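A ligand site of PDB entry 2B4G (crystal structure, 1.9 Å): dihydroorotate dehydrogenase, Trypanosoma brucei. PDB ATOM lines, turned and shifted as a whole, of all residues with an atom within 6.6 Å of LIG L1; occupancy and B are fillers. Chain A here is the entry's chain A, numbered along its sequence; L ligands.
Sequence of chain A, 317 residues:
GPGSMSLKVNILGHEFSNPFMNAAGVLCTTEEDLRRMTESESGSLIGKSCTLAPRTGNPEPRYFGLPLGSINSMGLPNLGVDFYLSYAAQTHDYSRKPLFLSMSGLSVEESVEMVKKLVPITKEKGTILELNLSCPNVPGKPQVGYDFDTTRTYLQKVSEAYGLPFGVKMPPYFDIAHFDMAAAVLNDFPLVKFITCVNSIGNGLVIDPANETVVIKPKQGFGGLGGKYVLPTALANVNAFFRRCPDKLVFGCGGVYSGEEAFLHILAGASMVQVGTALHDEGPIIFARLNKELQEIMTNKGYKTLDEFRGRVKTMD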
ATOM      1  N   ALA A  24      16.197 -16.084  21.476  1.00  0.00           N
ATOM      2  CA  ALA A  24      17.484 -16.654  21.905  1.00  0.00           C
ATOM      3  C   ALA A  24      18.048 -17.611  20.836  1.00  0.00           C
ATOM      4  O   ALA A  24      17.310 -18.380  20.214  1.00  0.00           O
ATOM      5  CB  ALA A  24      17.355 -17.347  23.246  1.00  0.00           C
ATOM      6  N   GLY A  25      19.347 -17.511  20.591  1.00  0.00           N
ATOM      7  CA  GLY A  25      20.031 -18.329  19.582  1.00  0.00           C
ATOM      8  C   GLY A  25      20.115 -17.774  18.173  1.00  0.00           C
ATOM      9  O   GLY A  25      20.936 -18.232  17.364  1.00  0.00           O
ATOM     10  N   LYS A  48      22.782 -15.722  23.172  1.00  0.00           N
ATOM     11  CA  LYS A  48      22.687 -17.151  22.888  1.00  0.00           C
ATOM     12  C   LYS A  48      22.634 -17.933  24.203  1.00  0.00           C
ATOM     13  O   LYS A  48      23.359 -17.602  25.150  1.00  0.00           O
ATOM     14  CB  LYS A  48      23.917 -17.588  22.059  1.00  0.00           C
ATOM     15  CG  LYS A  48      24.065 -19.106  21.831  1.00  0.00           C
ATOM     16  CD  LYS A  48      22.930 -19.703  20.972  1.00  0.00           C
ATOM     17  CE  LYS A  48      22.894 -21.245  21.054  1.00  0.00           C
ATOM     18  NZ  LYS A  48      21.930 -21.910  20.095  1.00  0.00           N
ATOM     19  N   SER A  49      21.773 -18.952  24.248  1.00  0.00           N
ATOM     20  CA  SER A  49      21.788 -19.887  25.371  1.00  0.00           C
ATOM     21  C   SER A  49      23.205 -20.421  25.542  1.00  0.00           C
ATOM     22  O   SER A  49      23.737 -21.059  24.631  1.00  0.00           O
ATOM     23  CB  SER A  49      20.843 -21.048  25.149  1.00  0.00           C
ATOM     24  OG  SER A  49      19.534 -20.671  25.475  1.00  0.00           O
ATOM     25  N   ASN A  58      26.444 -29.337  17.490  1.00  0.00           N
ATOM     26  CA  ASN A  58      26.218 -30.568  16.734  1.00  0.00           C
ATOM     27  C   ASN A  58      26.872 -30.498  15.329  1.00  0.00           C
ATOM     28  O   ASN A  58      27.206 -29.412  14.851  1.00  0.00           O
ATOM     29  CB  ASN A  58      24.715 -30.852  16.582  1.00  0.00           C
ATOM     30  CG  ASN A  58      24.043 -31.273  17.892  1.00  0.00           C
ATOM     31  OD1 ASN A  58      24.667 -31.822  18.801  1.00  0.00           O
ATOM     32  ND2 ASN A  58      22.739 -31.015  17.986  1.00  0.00           N
ATOM     33  N   ASN A  72      16.112 -26.858  13.018  1.00  0.00           N
ATOM     34  CA  ASN A  72      17.459 -26.696  13.552  1.00  0.00           C
ATOM     35  C   ASN A  72      17.777 -27.737  14.603  1.00  0.00           C
ATOM     36  O   ASN A  72      16.908 -28.118  15.393  1.00  0.00           O
ATOM     37  CB  ASN A  72      17.719 -25.278  14.118  1.00  0.00           C
ATOM     38  CG  ASN A  72      17.341 -25.134  15.600  1.00  0.00           C
ATOM     39  OD1 ASN A  72      18.129 -25.456  16.509  1.00  0.00           O
ATOM     40  ND2 ASN A  72      16.139 -24.641  15.844  1.00  0.00           N
ATOM     41  N   SER A  73      19.045 -28.155  14.611  1.00  0.00           N
ATOM     42  CA  SER A  73      19.591 -28.923  15.708  1.00  0.00           C
ATOM     43  C   SER A  73      20.994 -28.392  16.068  1.00  0.00           C
ATOM     44  O   SER A  73      21.993 -29.114  15.972  1.00  0.00           O
ATOM     45  CB  SER A  73      19.625 -30.405  15.349  1.00  0.00           C
ATOM     46  OG  SER A  73      19.959 -31.187  16.486  1.00  0.00           O
ATOM     47  N   MET A  74      21.081 -27.137  16.477  1.00  0.00           N
ATOM     48  CA  MET A  74      22.385 -26.480  16.675  1.00  0.00           C
ATOM     49  C   MET A  74      23.230 -27.213  17.722  1.00  0.00           C
ATOM     50  O   MET A  74      24.418 -27.430  17.518  1.00  0.00           O
ATOM     51  CB  MET A  74      22.214 -25.011  17.066  1.00  0.00           C
ATOM     52  CG  MET A  74      21.280 -24.184  16.185  1.00  0.00           C
ATOM     53  SD  MET A  74      21.671 -24.219  14.417  1.00  0.00           S
ATOM     54  CE  MET A  74      23.226 -23.329  14.402  1.00  0.00           C
ATOM     55  N   GLY A  75      22.610 -27.584  18.838  1.00  0.00           N
ATOM     56  CA  GLY A  75      23.275 -28.256  19.935  1.00  0.00           C
ATOM     57  C   GLY A  75      23.958 -27.281  20.873  1.00  0.00           C
ATOM     58  O   GLY A  75      24.988 -27.605  21.409  1.00  0.00           O
ATOM     59  N   LEU A  76      23.389 -26.088  21.043  1.00  0.00           N
ATOM     60  CA  LEU A  76      23.906 -25.063  21.947  1.00  0.00           C
ATOM     61  C   LEU A  76      25.373 -24.648  21.690  1.00  0.00           C
ATOM     62  O   LEU A  76      26.185 -24.587  22.611  1.00  0.00           O
ATOM     63  CB  LEU A  76      23.685 -25.463  23.414  1.00  0.00           C
ATOM     64  CG  LEU A  76      22.238 -25.631  23.893  1.00  0.00           C
ATOM     65  CD1 LEU A  76      22.218 -26.348  25.230  1.00  0.00           C
ATOM     66  CD2 LEU A  76      21.507 -24.300  24.018  1.00  0.00           C
ATOM     67  N   PRO A  77      25.725 -24.367  20.423  1.00  0.00           N
ATOM     68  CA  PRO A  77      27.046 -23.821  20.150  1.00  0.00           C
ATOM     69  C   PRO A  77      27.121 -22.416  20.735  1.00  0.00           C
ATOM     70  O   PRO A  77      26.259 -21.584  20.449  1.00  0.00           O
ATOM     71  CB  PRO A  77      27.118 -23.793  18.622  1.00  0.00           C
ATOM     72  CG  PRO A  77      25.696 -23.704  18.196  1.00  0.00           C
ATOM     73  CD  PRO A  77      24.913 -24.467  19.208  1.00  0.00           C
ATOM     74  N   SER A 104      21.584 -21.914  29.623  1.00  0.00           N
ATOM     75  CA  SER A 104      21.098 -23.259  29.321  1.00  0.00           C
ATOM     76  C   SER A 104      22.078 -24.326  29.824  1.00  0.00           C
ATOM     77  O   SER A 104      22.637 -25.094  29.060  1.00  0.00           O
ATOM     78  CB  SER A 104      20.854 -23.411  27.812  1.00  0.00           C
ATOM     79  OG  SER A 104      20.170 -24.613  27.492  1.00  0.00           O
ATOM     80  N   ASN A 132      16.659 -21.182  30.141  1.00  0.00           N
ATOM     81  CA  ASN A 132      16.190 -22.052  29.073  1.00  0.00           C
ATOM     82  C   ASN A 132      15.868 -23.436  29.621  1.00  0.00           C
ATOM     83  O   ASN A 132      16.737 -24.142  30.133  1.00  0.00           O
ATOM     84  CB  ASN A 132      17.207 -22.151  27.910  1.00  0.00           C
ATOM     85  CG  ASN A 132      16.654 -22.925  26.719  1.00  0.00           C
ATOM     86  OD1 ASN A 132      15.525 -23.441  26.732  1.00  0.00           O
ATOM     87  ND2 ASN A 132      17.479 -23.029  25.675  1.00  0.00           N
ATOM     88  N   SER A 134      13.952 -25.644  27.664  1.00  0.00           N
ATOM     89  CA  SER A 134      13.304 -26.285  26.516  1.00  0.00           C
ATOM     90  C   SER A 134      14.198 -26.550  25.290  1.00  0.00           C
ATOM     91  O   SER A 134      13.680 -26.643  24.176  1.00  0.00           O
ATOM     92  CB  SER A 134      12.077 -25.452  26.118  1.00  0.00           C
ATOM     93  OG  SER A 134      12.375 -24.059  26.151  1.00  0.00           O
ATOM     94  N   CYS A 135      15.506 -26.704  25.486  1.00  0.00           N
ATOM     95  CA  CYS A 135      16.386 -27.144  24.395  1.00  0.00           C
ATOM     96  C   CYS A 135      15.987 -28.533  23.931  1.00  0.00           C
ATOM     97  O   CYS A 135      16.069 -29.490  24.692  1.00  0.00           O
ATOM     98  CB  CYS A 135      17.861 -27.177  24.796  1.00  0.00           C
ATOM     99  SG  CYS A 135      18.903 -27.710  23.384  1.00  0.00           S
ATOM    100  N   PRO A 136      15.551 -28.670  22.663  1.00  0.00           N
ATOM    101  CA  PRO A 136      15.194 -29.996  22.180  1.00  0.00           C
ATOM    102  C   PRO A 136      16.270 -30.714  21.362  1.00  0.00           C
ATOM    103  O   PRO A 136      15.978 -31.729  20.704  1.00  0.00           O
ATOM    104  CB  PRO A 136      14.013 -29.687  21.277  1.00  0.00           C
ATOM    105  CG  PRO A 136      14.426 -28.383  20.611  1.00  0.00           C
ATOM    106  CD  PRO A 136      15.259 -27.642  21.635  1.00  0.00           C
ATOM    107  N   ASN A 137      17.512 -30.217  21.404  1.00  0.00           N
ATOM    108  CA  ASN A 137      18.546 -30.617  20.436  1.00  0.00           C
ATOM    109  C   ASN A 137      19.822 -31.266  20.976  1.00  0.00           C
ATOM    110  O   ASN A 137      20.744 -31.567  20.208  1.00  0.00           O
ATOM    111  CB  ASN A 137      18.889 -29.418  19.547  1.00  0.00           C
ATOM    112  CG  ASN A 137      17.725 -29.006  18.661  1.00  0.00           C
ATOM    113  OD1 ASN A 137      16.890 -29.828  18.289  1.00  0.00           O
ATOM    114  ND2 ASN A 137      17.664 -27.722  18.330  1.00  0.00           N
ATOM    115  N   VAL A 138      19.896 -31.500  22.279  1.00  0.00           N
ATOM    116  CA  VAL A 138      21.049 -32.186  22.866  1.00  0.00           C
ATOM    117  C   VAL A 138      20.669 -33.629  23.202  1.00  0.00           C
ATOM    118  O   VAL A 138      19.845 -33.832  24.075  1.00  0.00           O
ATOM    119  CB  VAL A 138      21.552 -31.499  24.148  1.00  0.00           C
ATOM    120  CG1 VAL A 138      22.950 -32.075  24.542  1.00  0.00           C
ATOM    121  CG2 VAL A 138      21.600 -29.974  23.970  1.00  0.00           C
ATOM    122  N   LYS A 169      12.116 -19.834  29.492  1.00  0.00           N
ATOM    123  CA  LYS A 169      11.814 -20.183  28.104  1.00  0.00           C
ATOM    124  C   LYS A 169      11.175 -21.555  28.161  1.00  0.00           C
ATOM    125  O   LYS A 169      11.822 -22.561  28.504  1.00  0.00           O
ATOM    126  CB  LYS A 169      13.097 -20.187  27.261  1.00  0.00           C
ATOM    127  CG  LYS A 169      12.903 -20.424  25.768  1.00  0.00           C
ATOM    128  CD  LYS A 169      12.192 -19.265  25.082  1.00  0.00           C
ATOM    129  CE  LYS A 169      12.149 -19.446  23.591  1.00  0.00           C
ATOM    130  NZ  LYS A 169      13.451 -19.203  22.924  1.00  0.00           N
ATOM    131  N   ASN A 199       9.584 -22.116  22.862  1.00  0.00           N
ATOM    132  CA  ASN A 199      10.720 -22.694  22.131  1.00  0.00           C
ATOM    133  C   ASN A 199      10.280 -23.456  20.874  1.00  0.00           C
ATOM    134  O   ASN A 199       9.084 -23.677  20.666  1.00  0.00           O
ATOM    135  CB  ASN A 199      11.565 -23.610  23.050  1.00  0.00           C
ATOM    136  CG  ASN A 199      13.052 -23.561  22.726  1.00  0.00           C
ATOM    137  OD1 ASN A 199      13.461 -23.746  21.580  1.00  0.00           O
ATOM    138  ND2 ASN A 199      13.866 -23.312  23.742  1.00  0.00           N
ATOM    139  N   SER A 200      11.225 -23.857  20.041  1.00  0.00           N
ATOM    140  CA  SER A 200      10.903 -24.591  18.811  1.00  0.00           C
ATOM    141  C   SER A 200      10.020 -25.823  19.062  1.00  0.00           C
ATOM    142  O   SER A 200      10.081 -26.426  20.135  1.00  0.00           O
ATOM    143  CB  SER A 200      12.202 -25.001  18.096  1.00  0.00           C
ATOM    144  OG  SER A 200      13.013 -25.788  18.932  1.00  0.00           O
ATOM    145  N   GLY A 224      14.285 -29.029  15.909  1.00  0.00           N
ATOM    146  CA  GLY A 224      13.220 -28.117  16.291  1.00  0.00           C
ATOM    147  C   GLY A 224      12.695 -27.272  15.143  1.00  0.00           C
ATOM    148  O   GLY A 224      13.467 -26.792  14.324  1.00  0.00           O
ATOM    149  N   LEU A 225      11.387 -27.090  15.106  1.00  0.00           N
ATOM    150  CA  LEU A 225      10.695 -26.327  14.048  1.00  0.00           C
ATOM    151  C   LEU A 225      10.358 -24.930  14.563  1.00  0.00           C
ATOM    152  O   LEU A 225       9.897 -24.773  15.692  1.00  0.00           O
ATOM    153  CB  LEU A 225       9.391 -27.022  13.656  1.00  0.00           C
ATOM    154  CG  LEU A 225       9.450 -28.436  13.103  1.00  0.00           C
ATOM    155  CD1 LEU A 225       8.026 -29.047  12.973  1.00  0.00           C
ATOM    156  CD2 LEU A 225      10.161 -28.437  11.753  1.00  0.00           C
HETATM  157  N1  LIG L   1      17.748 -24.822  19.352  1.00  0.00           N
HETATM  158  C1  LIG L   1      16.494 -24.503  19.645  1.00  0.00           C
HETATM  159  O1  LIG L   1      15.638 -24.509  18.718  1.00  0.00           O
HETATM  160  N2  LIG L   1      16.144 -24.196  20.908  1.00  0.00           N
HETATM  161  C2  LIG L   1      17.041 -24.204  21.910  1.00  0.00           C
HETATM  162  O2  LIG L   1      16.681 -23.913  23.089  1.00  0.00           O
HETATM  163  C3  LIG L   1      18.368 -24.558  21.617  1.00  0.00           C
HETATM  164  C4  LIG L   1      18.704 -24.864  20.302  1.00  0.00           C
HETATM  165  C5  LIG L   1      20.086 -25.323  19.892  1.00  0.00           C
HETATM  166  O3  LIG L   1      21.121 -24.768  20.285  1.00  0.00           O
HETATM  167  O4  LIG L   1      20.113 -26.359  19.155  1.00  0.00           O
HETATM  168  N1  LG2 L   2      15.930 -20.926  21.849  1.00  0.00           N
HETATM  169  C1  LG2 L   2      16.524 -20.841  23.068  1.00  0.00           C
HETATM  170  O1  LG2 L   2      15.833 -20.689  24.082  1.00  0.00           O
HETATM  171  N2  LG2 L   2      17.895 -20.929  23.155  1.00  0.00           N
HETATM  172  C2  LG2 L   2      18.700 -21.087  22.051  1.00  0.00           C
HETATM  173  O2  LG2 L   2      19.897 -20.825  22.173  1.00  0.00           O
HETATM  174  C3  LG2 L   2      18.102 -21.168  20.809  1.00  0.00           C
HETATM  175  N3  LG2 L   2      18.834 -21.350  19.667  1.00  0.00           N
HETATM  176  C4  LG2 L   2      18.218 -21.389  18.442  1.00  0.00           C
HETATM  177  C5  LG2 L   2      18.972 -21.526  17.270  1.00  0.00           C
HETATM  178  C6  LG2 L   2      18.346 -21.590  16.026  1.00  0.00           C
HETATM  179  C7  LG2 L   2      19.183 -21.388  14.779  1.00  0.00           C
HETATM  180  C8  LG2 L   2      16.944 -21.495  15.957  1.00  0.00           C
HETATM  181  C9  LG2 L   2      16.253 -21.034  14.694  1.00  0.00           C
HETATM  182  C10 LG2 L   2      16.208 -21.345  17.128  1.00  0.00           C
HETATM  183  C11 LG2 L   2      16.817 -21.271  18.364  1.00  0.00           C
HETATM  184  N4  LG2 L   2      16.059 -21.153  19.521  1.00  0.00           N
HETATM  185  C12 LG2 L   2      16.696 -21.092  20.725  1.00  0.00           C
HETATM  186  C13 LG2 L   2      14.555 -21.214  19.512  1.00  0.00           C
HETATM  187  C14 LG2 L   2      14.058 -19.796  19.245  1.00  0.00           C
HETATM  188  O3  LG2 L   2      14.541 -18.950  20.274  1.00  0.00           O
HETATM  189  C15 LG2 L   2      12.539 -19.732  19.127  1.00  0.00           C
HETATM  190  O4  LG2 L   2      11.946 -20.133  20.343  1.00  0.00           O
HETATM  191  C16 LG2 L   2      11.982 -20.607  17.992  1.00  0.00           C
HETATM  192  O5  LG2 L   2      12.891 -20.621  16.918  1.00  0.00           O
HETATM  193  C17 LG2 L   2      10.617 -20.166  17.468  1.00  0.00           C
HETATM  194  O6  LG2 L   2      10.553 -18.811  17.085  1.00  0.00           O
HETATM  195  P1  LG2 L   2      10.537 -18.412  15.535  1.00  0.00           P
HETATM  196  O7  LG2 L   2       9.327 -19.014  14.863  1.00  0.00           O
HETATM  197  O8  LG2 L   2      11.766 -19.021  14.914  1.00  0.00           O
HETATM  198  O9  LG2 L   2      10.537 -16.914  15.431  1.00  0.00           O
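The backbone NH (N) of Ser 49 sits close to an oxygen (O2) of LG2 L2, at 3.4 Å.
An oxygen (O3) of LIG L1 lies within salt-bridge range of the side-chain amino group (NZ) of Lys 48, at 3.0 Å.
N of Leu 76 sits at hydrogen-bond distance from O3 of LIG L1, 2.7 Å away.
ND2 of Asn 199 sits at hydrogen-bond distance from O1 of LG2 L2 (3.3 Å).
An oxygen (O3) of LG2 L2 sits at hydrogen-bond distance from the backbone carbonyl oxygen of Ala 24.
The side-chain amide nitrogen (ND2) of Asn 137 sits at hydrogen-bond distance from an oxygen (O4) of LIG L1, at 2.9 Å.
ND2 of Asn 132 is in hydrogen-bond range of O2 of LIG L1 (2.8 Å).
NZ of Lys 169 sits at hydrogen-bond distance from O3 of LG2 L2, 2.9 Å away.
The backbone NH (N) of Gly 75 is in hydrogen-bond range of an oxygen (O4) of LIG L1 (2.8 Å).
The side-chain amino group (NZ) of Lys 48 sits at hydrogen-bond distance from an oxygen (O2) of LG2 L2, 3.1 Å away.
The side-chain hydroxyl of Ser 49 lies within hydrogen-bond range of a nitrogen (N2) of LG2 L2 (2.9 Å).
The side-chain hydroxyl (OG) of Ser 200 lies within hydrogen-bond range of an oxygen (O1) of LIG L1, 2.9 Å away.
N of Met 74 is in hydrogen-bond range of O4 of LIG L1 (3.0 Å).
The side-chain amide oxygen (OD1) of Asn 199 is in hydrogen-bond range of a nitrogen (N2) of LIG L1 (2.8 Å).
An oxygen (O1) of LIG L1 sits at hydrogen-bond distance from the side-chain amide nitrogen (ND2) of Asn 72 (2.9 Å).
An oxygen (O1) of LG2 L2 lies within hydrogen-bond range of the side-chain amide nitrogen (ND2) of Asn 132 (3.3 Å).
Residues that only touch LIG L1: Cys 135, Pro 136, Ser 73 and Pro 77.
Within 4 Å of LIG L1: Lys 48, Asn 72, Ser 73, Met 74, Gly 75, Leu 76, Pro 77, Asn 132, Cys 135, Pro 136, Asn 137, Asn 199 and Ser 200.
The nearest printed residue that does not touch LIG L1 is Ser 134 (4.2 Å).
ND2 of Asn 58 is in hydrogen-bond range of O of Ser 73, 2.9 Å away.
The side-chain amide oxygen (OD1) of Asn 72 is in hydrogen-bond range of the side-chain amide nitrogen (ND2) of Asn 137 (2.9 Å).
The backbone NH of Asn 137 sits close to the side-chain sulfur of Cys 135 (3.5 Å).
O of Asn 137 sits at hydrogen-bond distance from ND2 of Asn 58 (3.0 Å).
The side-chain amide nitrogen of Asn 199 sits at hydrogen-bond distance from the side-chain hydroxyl of Ser 134 (2.9 Å).
O of Met 74 lies within hydrogen-bond range of N of Asn 58 (2.8 Å).
N of Cys 135 is in hydrogen-bond range of OD1 of Asn 132.
The side-chain amide oxygen (OD1) of Asn 199 is in hydrogen-bond range of the side-chain hydroxyl (OG) of Ser 200.
An oxygen (O2) of LIG L1 sits close to a nitrogen (N2) of LG2 L2 (3.2 Å).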
